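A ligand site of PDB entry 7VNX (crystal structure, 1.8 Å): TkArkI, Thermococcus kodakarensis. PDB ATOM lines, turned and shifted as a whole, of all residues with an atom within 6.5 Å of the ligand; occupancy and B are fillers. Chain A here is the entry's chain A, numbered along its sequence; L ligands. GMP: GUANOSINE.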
ATOM      1  N   LEU A  37       9.004  14.245   3.819  1.00  0.00           N
ATOM      2  CA  LEU A  37       8.585  13.098   4.617  1.00  0.00           C
ATOM      3  C   LEU A  37       9.192  11.792   4.135  1.00  0.00           C
ATOM      4  O   LEU A  37       9.722  11.028   4.956  1.00  0.00           O
ATOM      5  CB  LEU A  37       7.053  12.993   4.625  1.00  0.00           C
ATOM      6  CG  LEU A  37       6.465  11.864   5.503  1.00  0.00           C
ATOM      7  CD1 LEU A  37       6.894  12.009   6.972  1.00  0.00           C
ATOM      8  CD2 LEU A  37       4.949  11.793   5.381  1.00  0.00           C
ATOM      9  N   ALA A  38       9.138  11.497   2.837  1.00  0.00           N
ATOM     10  CA  ALA A  38       9.709  10.237   2.345  1.00  0.00           C
ATOM     11  C   ALA A  38       9.904  10.327   0.827  1.00  0.00           C
ATOM     12  O   ALA A  38       9.291  11.156   0.144  1.00  0.00           O
ATOM     13  CB  ALA A  38       8.801   9.053   2.718  1.00  0.00           C
ATOM     14  N   VAL A  45       7.364  12.709  -1.128  1.00  0.00           N
ATOM     15  CA  VAL A  45       6.272  12.902  -0.168  1.00  0.00           C
ATOM     16  C   VAL A  45       6.705  13.965   0.845  1.00  0.00           C
ATOM     17  O   VAL A  45       7.821  13.938   1.359  1.00  0.00           O
ATOM     18  CB  VAL A  45       5.859  11.597   0.533  1.00  0.00           C
ATOM     19  CG1 VAL A  45       4.575  11.829   1.341  1.00  0.00           C
ATOM     20  CG2 VAL A  45       5.611  10.480  -0.490  1.00  0.00           C
ATOM     21  N   THR A  47       5.054  16.715   4.158  1.00  0.00           N
ATOM     22  CA  THR A  47       3.922  17.138   4.996  1.00  0.00           C
ATOM     23  C   THR A  47       3.814  18.669   4.961  1.00  0.00           C
ATOM     24  O   THR A  47       4.766  19.379   4.605  1.00  0.00           O
ATOM     25  CB  THR A  47       4.071  16.634   6.442  1.00  0.00           C
ATOM     26  OG1 THR A  47       5.298  17.114   6.995  1.00  0.00           O
ATOM     27  CG2 THR A  47       4.080  15.127   6.543  1.00  0.00           C
ATOM     28  N   VAL A  56      -0.663  15.778   3.750  1.00  0.00           N
ATOM     29  CA  VAL A  56       0.418  15.084   3.066  1.00  0.00           C
ATOM     30  C   VAL A  56       0.354  15.482   1.596  1.00  0.00           C
ATOM     31  O   VAL A  56      -0.732  15.516   1.005  1.00  0.00           O
ATOM     32  CB  VAL A  56       0.309  13.544   3.218  1.00  0.00           C
ATOM     33  CG1 VAL A  56       1.330  12.772   2.337  1.00  0.00           C
ATOM     34  CG2 VAL A  56       0.475  13.189   4.721  1.00  0.00           C
ATOM     35  N   PRO A  86      -7.187   8.353   3.819  1.00  0.00           N
ATOM     36  CA  PRO A  86      -7.691   9.649   4.254  1.00  0.00           C
ATOM     37  C   PRO A  86      -8.076  10.488   3.055  1.00  0.00           C
ATOM     38  O   PRO A  86      -7.534  10.315   1.946  1.00  0.00           O
ATOM     39  CB  PRO A  86      -6.524  10.258   5.039  1.00  0.00           C
ATOM     40  CG  PRO A  86      -5.649   9.154   5.402  1.00  0.00           C
ATOM     41  CD  PRO A  86      -5.809   8.122   4.278  1.00  0.00           C
ATOM     42  N   ARG A 102      -3.572  15.191   0.512  1.00  0.00           N
ATOM     43  CA  ARG A 102      -4.605  14.484   1.265  1.00  0.00           C
ATOM     44  C   ARG A 102      -4.488  14.820   2.742  1.00  0.00           C
ATOM     45  O   ARG A 102      -3.455  15.320   3.212  1.00  0.00           O
ATOM     46  CB  ARG A 102      -4.483  12.960   1.058  1.00  0.00           C
ATOM     47  CG  ARG A 102      -3.166  12.409   1.584  1.00  0.00           C
ATOM     48  CD  ARG A 102      -3.311  10.971   2.019  1.00  0.00           C
ATOM     49  NE  ARG A 102      -2.044  10.317   2.301  1.00  0.00           N
ATOM     50  CZ  ARG A 102      -1.527  10.115   3.510  1.00  0.00           C
ATOM     51  NH1 ARG A 102      -2.161  10.534   4.610  1.00  0.00           N
ATOM     52  NH2 ARG A 102      -0.367   9.454   3.633  1.00  0.00           N
ATOM     53  N   GLU A 103      -5.535  14.481   3.503  1.00  0.00           N
ATOM     54  CA  GLU A 103      -5.475  14.736   4.937  1.00  0.00           C
ATOM     55  C   GLU A 103      -4.422  13.833   5.566  1.00  0.00           C
ATOM     56  O   GLU A 103      -4.204  12.694   5.132  1.00  0.00           O
ATOM     57  CB  GLU A 103      -6.824  14.465   5.603  1.00  0.00           C
ATOM     58  CG  GLU A 103      -7.963  15.226   5.004  1.00  0.00           C
ATOM     59  CD  GLU A 103      -8.101  16.598   5.629  1.00  0.00           C
ATOM     60  OE1 GLU A 103      -9.097  17.304   5.335  1.00  0.00           O
ATOM     61  OE2 GLU A 103      -7.238  16.956   6.437  1.00  0.00           O
ATOM     62  N   PHE A 104      -3.780  14.344   6.599  1.00  0.00           N
ATOM     63  CA  PHE A 104      -2.860  13.550   7.392  1.00  0.00           C
ATOM     64  C   PHE A 104      -3.688  12.911   8.501  1.00  0.00           C
ATOM     65  O   PHE A 104      -4.323  13.632   9.277  1.00  0.00           O
ATOM     66  CB  PHE A 104      -1.769  14.436   7.993  1.00  0.00           C
ATOM     67  CG  PHE A 104      -0.761  13.697   8.848  1.00  0.00           C
ATOM     68  CD1 PHE A 104      -0.953  13.574  10.216  1.00  0.00           C
ATOM     69  CD2 PHE A 104       0.376  13.136   8.288  1.00  0.00           C
ATOM     70  CE1 PHE A 104      -0.030  12.892  11.006  1.00  0.00           C
ATOM     71  CE2 PHE A 104       1.301  12.481   9.067  1.00  0.00           C
ATOM     72  CZ  PHE A 104       1.098  12.350  10.433  1.00  0.00           C
ATOM     73  N   ALA A 105      -3.624  11.591   8.607  1.00  0.00           N
ATOM     74  CA  ALA A 105      -4.371  10.871   9.637  1.00  0.00           C
ATOM     75  C   ALA A 105      -3.550  10.799  10.922  1.00  0.00           C
ATOM     76  O   ALA A 105      -2.469  10.210  10.942  1.00  0.00           O
ATOM     77  CB  ALA A 105      -4.700   9.464   9.118  1.00  0.00           C
ATOM     78  N   GLU A 106      -4.027  11.445  11.992  1.00  0.00           N
ATOM     79  CA  GLU A 106      -3.266  11.424  13.241  1.00  0.00           C
ATOM     80  C   GLU A 106      -3.349  10.030  13.846  1.00  0.00           C
ATOM     81  O   GLU A 106      -4.341   9.317  13.683  1.00  0.00           O
ATOM     82  CB  GLU A 106      -3.767  12.502  14.205  1.00  0.00           C
ATOM     83  CG  GLU A 106      -3.572  13.958  13.685  1.00  0.00           C
ATOM     84  CD  GLU A 106      -2.116  14.457  13.725  1.00  0.00           C
ATOM     85  OE1 GLU A 106      -1.260  13.818  14.375  1.00  0.00           O
ATOM     86  OE2 GLU A 106      -1.823  15.515  13.108  1.00  0.00           O
ATOM     87  N   GLY A 107      -2.264   9.610  14.478  1.00  0.00           N
ATOM     88  CA  GLY A 107      -2.209   8.244  14.962  1.00  0.00           C
ATOM     89  C   GLY A 107      -0.854   7.654  14.644  1.00  0.00           C
ATOM     90  O   GLY A 107       0.102   8.365  14.311  1.00  0.00           O
ATOM     91  N   GLU A 108      -0.749   6.346  14.807  1.00  0.00           N
ATOM     92  CA  GLU A 108       0.503   5.646  14.703  1.00  0.00           C
ATOM     93  C   GLU A 108       0.326   4.547  13.660  1.00  0.00           C
ATOM     94  O   GLU A 108      -0.753   3.955  13.562  1.00  0.00           O
ATOM     95  CB  GLU A 108       0.868   4.976  16.028  1.00  0.00           C
ATOM     96  CG  GLU A 108       1.243   5.990  17.101  1.00  0.00           C
ATOM     97  CD  GLU A 108       2.543   6.649  16.733  1.00  0.00           C
ATOM     98  OE1 GLU A 108       3.445   5.934  16.222  1.00  0.00           O
ATOM     99  OE2 GLU A 108       2.666   7.877  16.921  1.00  0.00           O
ATOM    100  N   PRO A 109       1.364   4.256  12.892  1.00  0.00           N
ATOM    101  CA  PRO A 109       1.330   3.032  12.087  1.00  0.00           C
ATOM    102  C   PRO A 109       1.194   1.814  12.992  1.00  0.00           C
ATOM    103  O   PRO A 109       1.639   1.844  14.139  1.00  0.00           O
ATOM    104  CB  PRO A 109       2.686   3.060  11.339  1.00  0.00           C
ATOM    105  CG  PRO A 109       3.502   4.051  12.049  1.00  0.00           C
ATOM    106  CD  PRO A 109       2.623   5.011  12.772  1.00  0.00           C
ATOM    107  N   PHE A 112       3.745   0.369  15.308  1.00  0.00           N
ATOM    108  CA  PHE A 112       4.072   1.000  16.583  1.00  0.00           C
ATOM    109  C   PHE A 112       2.854   1.285  17.443  1.00  0.00           C
ATOM    110  O   PHE A 112       2.995   1.934  18.488  1.00  0.00           O
ATOM    111  CB  PHE A 112       4.817   2.322  16.368  1.00  0.00           C
ATOM    112  CG  PHE A 112       6.065   2.190  15.578  1.00  0.00           C
ATOM    113  CD1 PHE A 112       7.112   1.413  16.056  1.00  0.00           C
ATOM    114  CD2 PHE A 112       6.204   2.831  14.369  1.00  0.00           C
ATOM    115  CE1 PHE A 112       8.287   1.278  15.326  1.00  0.00           C
ATOM    116  CE2 PHE A 112       7.376   2.683  13.622  1.00  0.00           C
ATOM    117  CZ  PHE A 112       8.412   1.907  14.102  1.00  0.00           C
ATOM    118  N   GLY A 143       3.618  -3.386   8.498  1.00  0.00           N
ATOM    119  CA  GLY A 143       2.865  -2.567   9.431  1.00  0.00           C
ATOM    120  C   GLY A 143       3.065  -1.081   9.312  1.00  0.00           C
ATOM    121  O   GLY A 143       2.656  -0.341  10.220  1.00  0.00           O
ATOM    122  N   LYS A 144       3.683  -0.605   8.235  1.00  0.00           N
ATOM    123  CA  LYS A 144       3.951   0.813   8.089  1.00  0.00           C
ATOM    124  C   LYS A 144       2.884   1.553   7.307  1.00  0.00           C
ATOM    125  O   LYS A 144       2.956   2.790   7.227  1.00  0.00           O
ATOM    126  CB  LYS A 144       5.314   1.037   7.422  1.00  0.00           C
ATOM    127  CG  LYS A 144       6.447   0.545   8.292  1.00  0.00           C
ATOM    128  CD  LYS A 144       7.799   0.962   7.794  1.00  0.00           C
ATOM    129  CE  LYS A 144       8.890   0.335   8.637  1.00  0.00           C
ATOM    130  NZ  LYS A 144      10.258   0.683   8.161  1.00  0.00           N
ATOM    131  N   HIS A 145       1.912   0.839   6.742  1.00  0.00           N
ATOM    132  CA  HIS A 145       0.926   1.424   5.825  1.00  0.00           C
ATOM    133  C   HIS A 145      -0.499   1.323   6.322  1.00  0.00           C
ATOM    134  O   HIS A 145      -1.411   1.585   5.545  1.00  0.00           O
ATOM    135  CB  HIS A 145       1.036   0.759   4.437  1.00  0.00           C
ATOM    136  CG  HIS A 145       2.386   0.910   3.814  1.00  0.00           C
ATOM    137  ND1 HIS A 145       3.452   0.096   4.117  1.00  0.00           N
ATOM    138  CD2 HIS A 145       2.862   1.812   2.917  1.00  0.00           C
ATOM    139  CE1 HIS A 145       4.517   0.472   3.439  1.00  0.00           C
ATOM    140  NE2 HIS A 145       4.190   1.523   2.710  1.00  0.00           N
ATOM    141  N   ILE A 147      -2.647   3.009   9.393  1.00  0.00           N
ATOM    142  CA  ILE A 147      -2.543   4.027  10.427  1.00  0.00           C
ATOM    143  C   ILE A 147      -3.679   3.821  11.425  1.00  0.00           C
ATOM    144  O   ILE A 147      -4.853   3.729  11.028  1.00  0.00           O
ATOM    145  CB  ILE A 147      -2.589   5.441   9.832  1.00  0.00           C
ATOM    146  CG1 ILE A 147      -1.458   5.620   8.822  1.00  0.00           C
ATOM    147  CG2 ILE A 147      -2.534   6.454  10.946  1.00  0.00           C
ATOM    148  CD1 ILE A 147      -0.070   5.261   9.386  1.00  0.00           C
ATOM    149  N   ILE A 148      -3.326   3.768  12.698  1.00  0.00           N
ATOM    150  CA  ILE A 148      -4.282   3.525  13.772  1.00  0.00           C
ATOM    151  C   ILE A 148      -4.525   4.859  14.478  1.00  0.00           C
ATOM    152  O   ILE A 148      -3.642   5.355  15.170  1.00  0.00           O
ATOM    153  CB  ILE A 148      -3.743   2.474  14.757  1.00  0.00           C
ATOM    154  CG1 ILE A 148      -3.387   1.192  14.010  1.00  0.00           C
ATOM    155  CG2 ILE A 148      -4.721   2.236  15.881  1.00  0.00           C
ATOM    156  CD1 ILE A 148      -4.600   0.474  13.411  1.00  0.00           C
ATOM    157  N   ILE A 155      -2.659   3.585   3.754  1.00  0.00           N
ATOM    158  CA  ILE A 155      -2.033   4.674   3.020  1.00  0.00           C
ATOM    159  C   ILE A 155      -1.036   4.125   2.001  1.00  0.00           C
ATOM    160  O   ILE A 155      -0.570   2.992   2.112  1.00  0.00           O
ATOM    161  CB  ILE A 155      -1.322   5.679   3.967  1.00  0.00           C
ATOM    162  CG1 ILE A 155      -0.327   4.981   4.909  1.00  0.00           C
ATOM    163  CG2 ILE A 155      -2.373   6.528   4.788  1.00  0.00           C
ATOM    164  CD1 ILE A 155       0.644   5.967   5.635  1.00  0.00           C
ATOM    165  N   ASP A 156      -0.659   4.974   1.045  1.00  0.00           N
ATOM    166  CA  ASP A 156       0.492   4.728   0.177  1.00  0.00           C
ATOM    167  C   ASP A 156       0.246   3.567  -0.800  1.00  0.00           C
ATOM    168  O   ASP A 156       0.580   2.419  -0.474  1.00  0.00           O
ATOM    169  CB  ASP A 156       1.744   4.453   0.982  1.00  0.00           C
ATOM    170  CG  ASP A 156       2.295   5.694   1.624  1.00  0.00           C
ATOM    171  OD1 ASP A 156       1.957   6.815   1.163  1.00  0.00           O
ATOM    172  OD2 ASP A 156       3.069   5.551   2.592  1.00  0.00           O
ATOM    173  N   GLU A 158       1.413   2.852  -3.820  1.00  0.00           N
ATOM    174  CA  GLU A 158       2.384   2.741  -4.907  1.00  0.00           C
ATOM    175  C   GLU A 158       2.491   1.314  -5.422  1.00  0.00           C
ATOM    176  O   GLU A 158       2.887   1.101  -6.580  1.00  0.00           O
ATOM    177  CB  GLU A 158       3.780   3.191  -4.485  1.00  0.00           C
ATOM    178  CG  GLU A 158       3.856   4.432  -3.687  1.00  0.00           C
ATOM    179  CD  GLU A 158       3.648   4.143  -2.217  1.00  0.00           C
ATOM    180  OE1 GLU A 158       4.208   3.136  -1.734  1.00  0.00           O
ATOM    181  OE2 GLU A 158       2.909   4.917  -1.561  1.00  0.00           O
HETATM  182  O5' GMP L   1       4.457   6.766   4.385  1.00  0.00           O
HETATM  183  C5' GMP L   1       5.198   5.916   5.256  1.00  0.00           C
HETATM  184  C4' GMP L   1       5.210   6.468   6.668  1.00  0.00           C
HETATM  185  O4' GMP L   1       4.897   7.885   6.654  1.00  0.00           O
HETATM  186  C3' GMP L   1       4.199   5.858   7.620  1.00  0.00           C
HETATM  187  O3' GMP L   1       4.602   4.601   8.155  1.00  0.00           O
HETATM  188  C2' GMP L   1       4.010   6.961   8.666  1.00  0.00           C
HETATM  189  O2' GMP L   1       5.092   6.982   9.582  1.00  0.00           O
HETATM  190  C1' GMP L   1       4.103   8.207   7.790  1.00  0.00           C
HETATM  191  N9  GMP L   1       2.775   8.663   7.332  1.00  0.00           N
HETATM  192  C8  GMP L   1       2.386   8.909   6.065  1.00  0.00           C
HETATM  193  N7  GMP L   1       1.091   9.318   5.993  1.00  0.00           N
HETATM  194  C5  GMP L   1       0.635   9.326   7.260  1.00  0.00           C
HETATM  195  C6  GMP L   1      -0.641   9.646   7.919  1.00  0.00           C
HETATM  196  O6  GMP L   1      -1.622  10.038   7.254  1.00  0.00           O
HETATM  197  N1  GMP L   1      -0.704   9.520   9.263  1.00  0.00           N
HETATM  198  C2  GMP L   1       0.335   9.134  10.037  1.00  0.00           C
HETATM  199  N2  GMP L   1       0.157   9.062  11.384  1.00  0.00           N
HETATM  200  N3  GMP L   1       1.534   8.805   9.480  1.00  0.00           N
HETATM  201  C4  GMP L   1       1.745   8.891   8.136  1.00  0.00           C
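The side-chain carboxylate (OD2) of Asp 156 is in hydrogen-bond range of an oxygen (O5') of the ligand, at 2.6 Å.
N2 of the ligand sits at hydrogen-bond distance from O of Gly 107, 3.0 Å away.
The backbone carbonyl oxygen (O) of Ala 105 sits at hydrogen-bond distance from a nitrogen (N1) of the ligand, 2.5 Å away.
O of Lys 144 lies within hydrogen-bond range of O3' of the ligand (2.6 Å).
N of Ala 105 sits at hydrogen-bond distance from O6 of the ligand, at 2.9 Å.
The guanidinium group (NH1) of Arg 102 sits at hydrogen-bond distance from an oxygen (O6) of the ligand (2.7 Å).
The backbone NH of Val 56 sits at hydrogen-bond distance from the backbone carbonyl oxygen of Arg 102, at 2.9 Å.
The backbone NH of Ile 155 sits at hydrogen-bond distance from the backbone carbonyl oxygen of His 145 (3.0 Å).
N of Leu 37 lies within hydrogen-bond range of O of Val 45, 2.7 Å away.
CD2 of Leu 37 touches C8 of the ligand (3.9 Å).
CZ of Phe 104 touches C2 of the ligand, 3.3 Å away.
Ile 147 touches the ligand.
Ile 155 touches the ligand.
Hydrophobic or aromatic side chains within 4 Å of the ligand: Leu 37, Phe 104, Ala 105, Ile 147 and Ile 155.
Along chain A the residues within 4 Å of the ligand span positions 37 to 156.
The nearest printed residue that does not touch the ligand is Pro 109 (4.02 Å).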
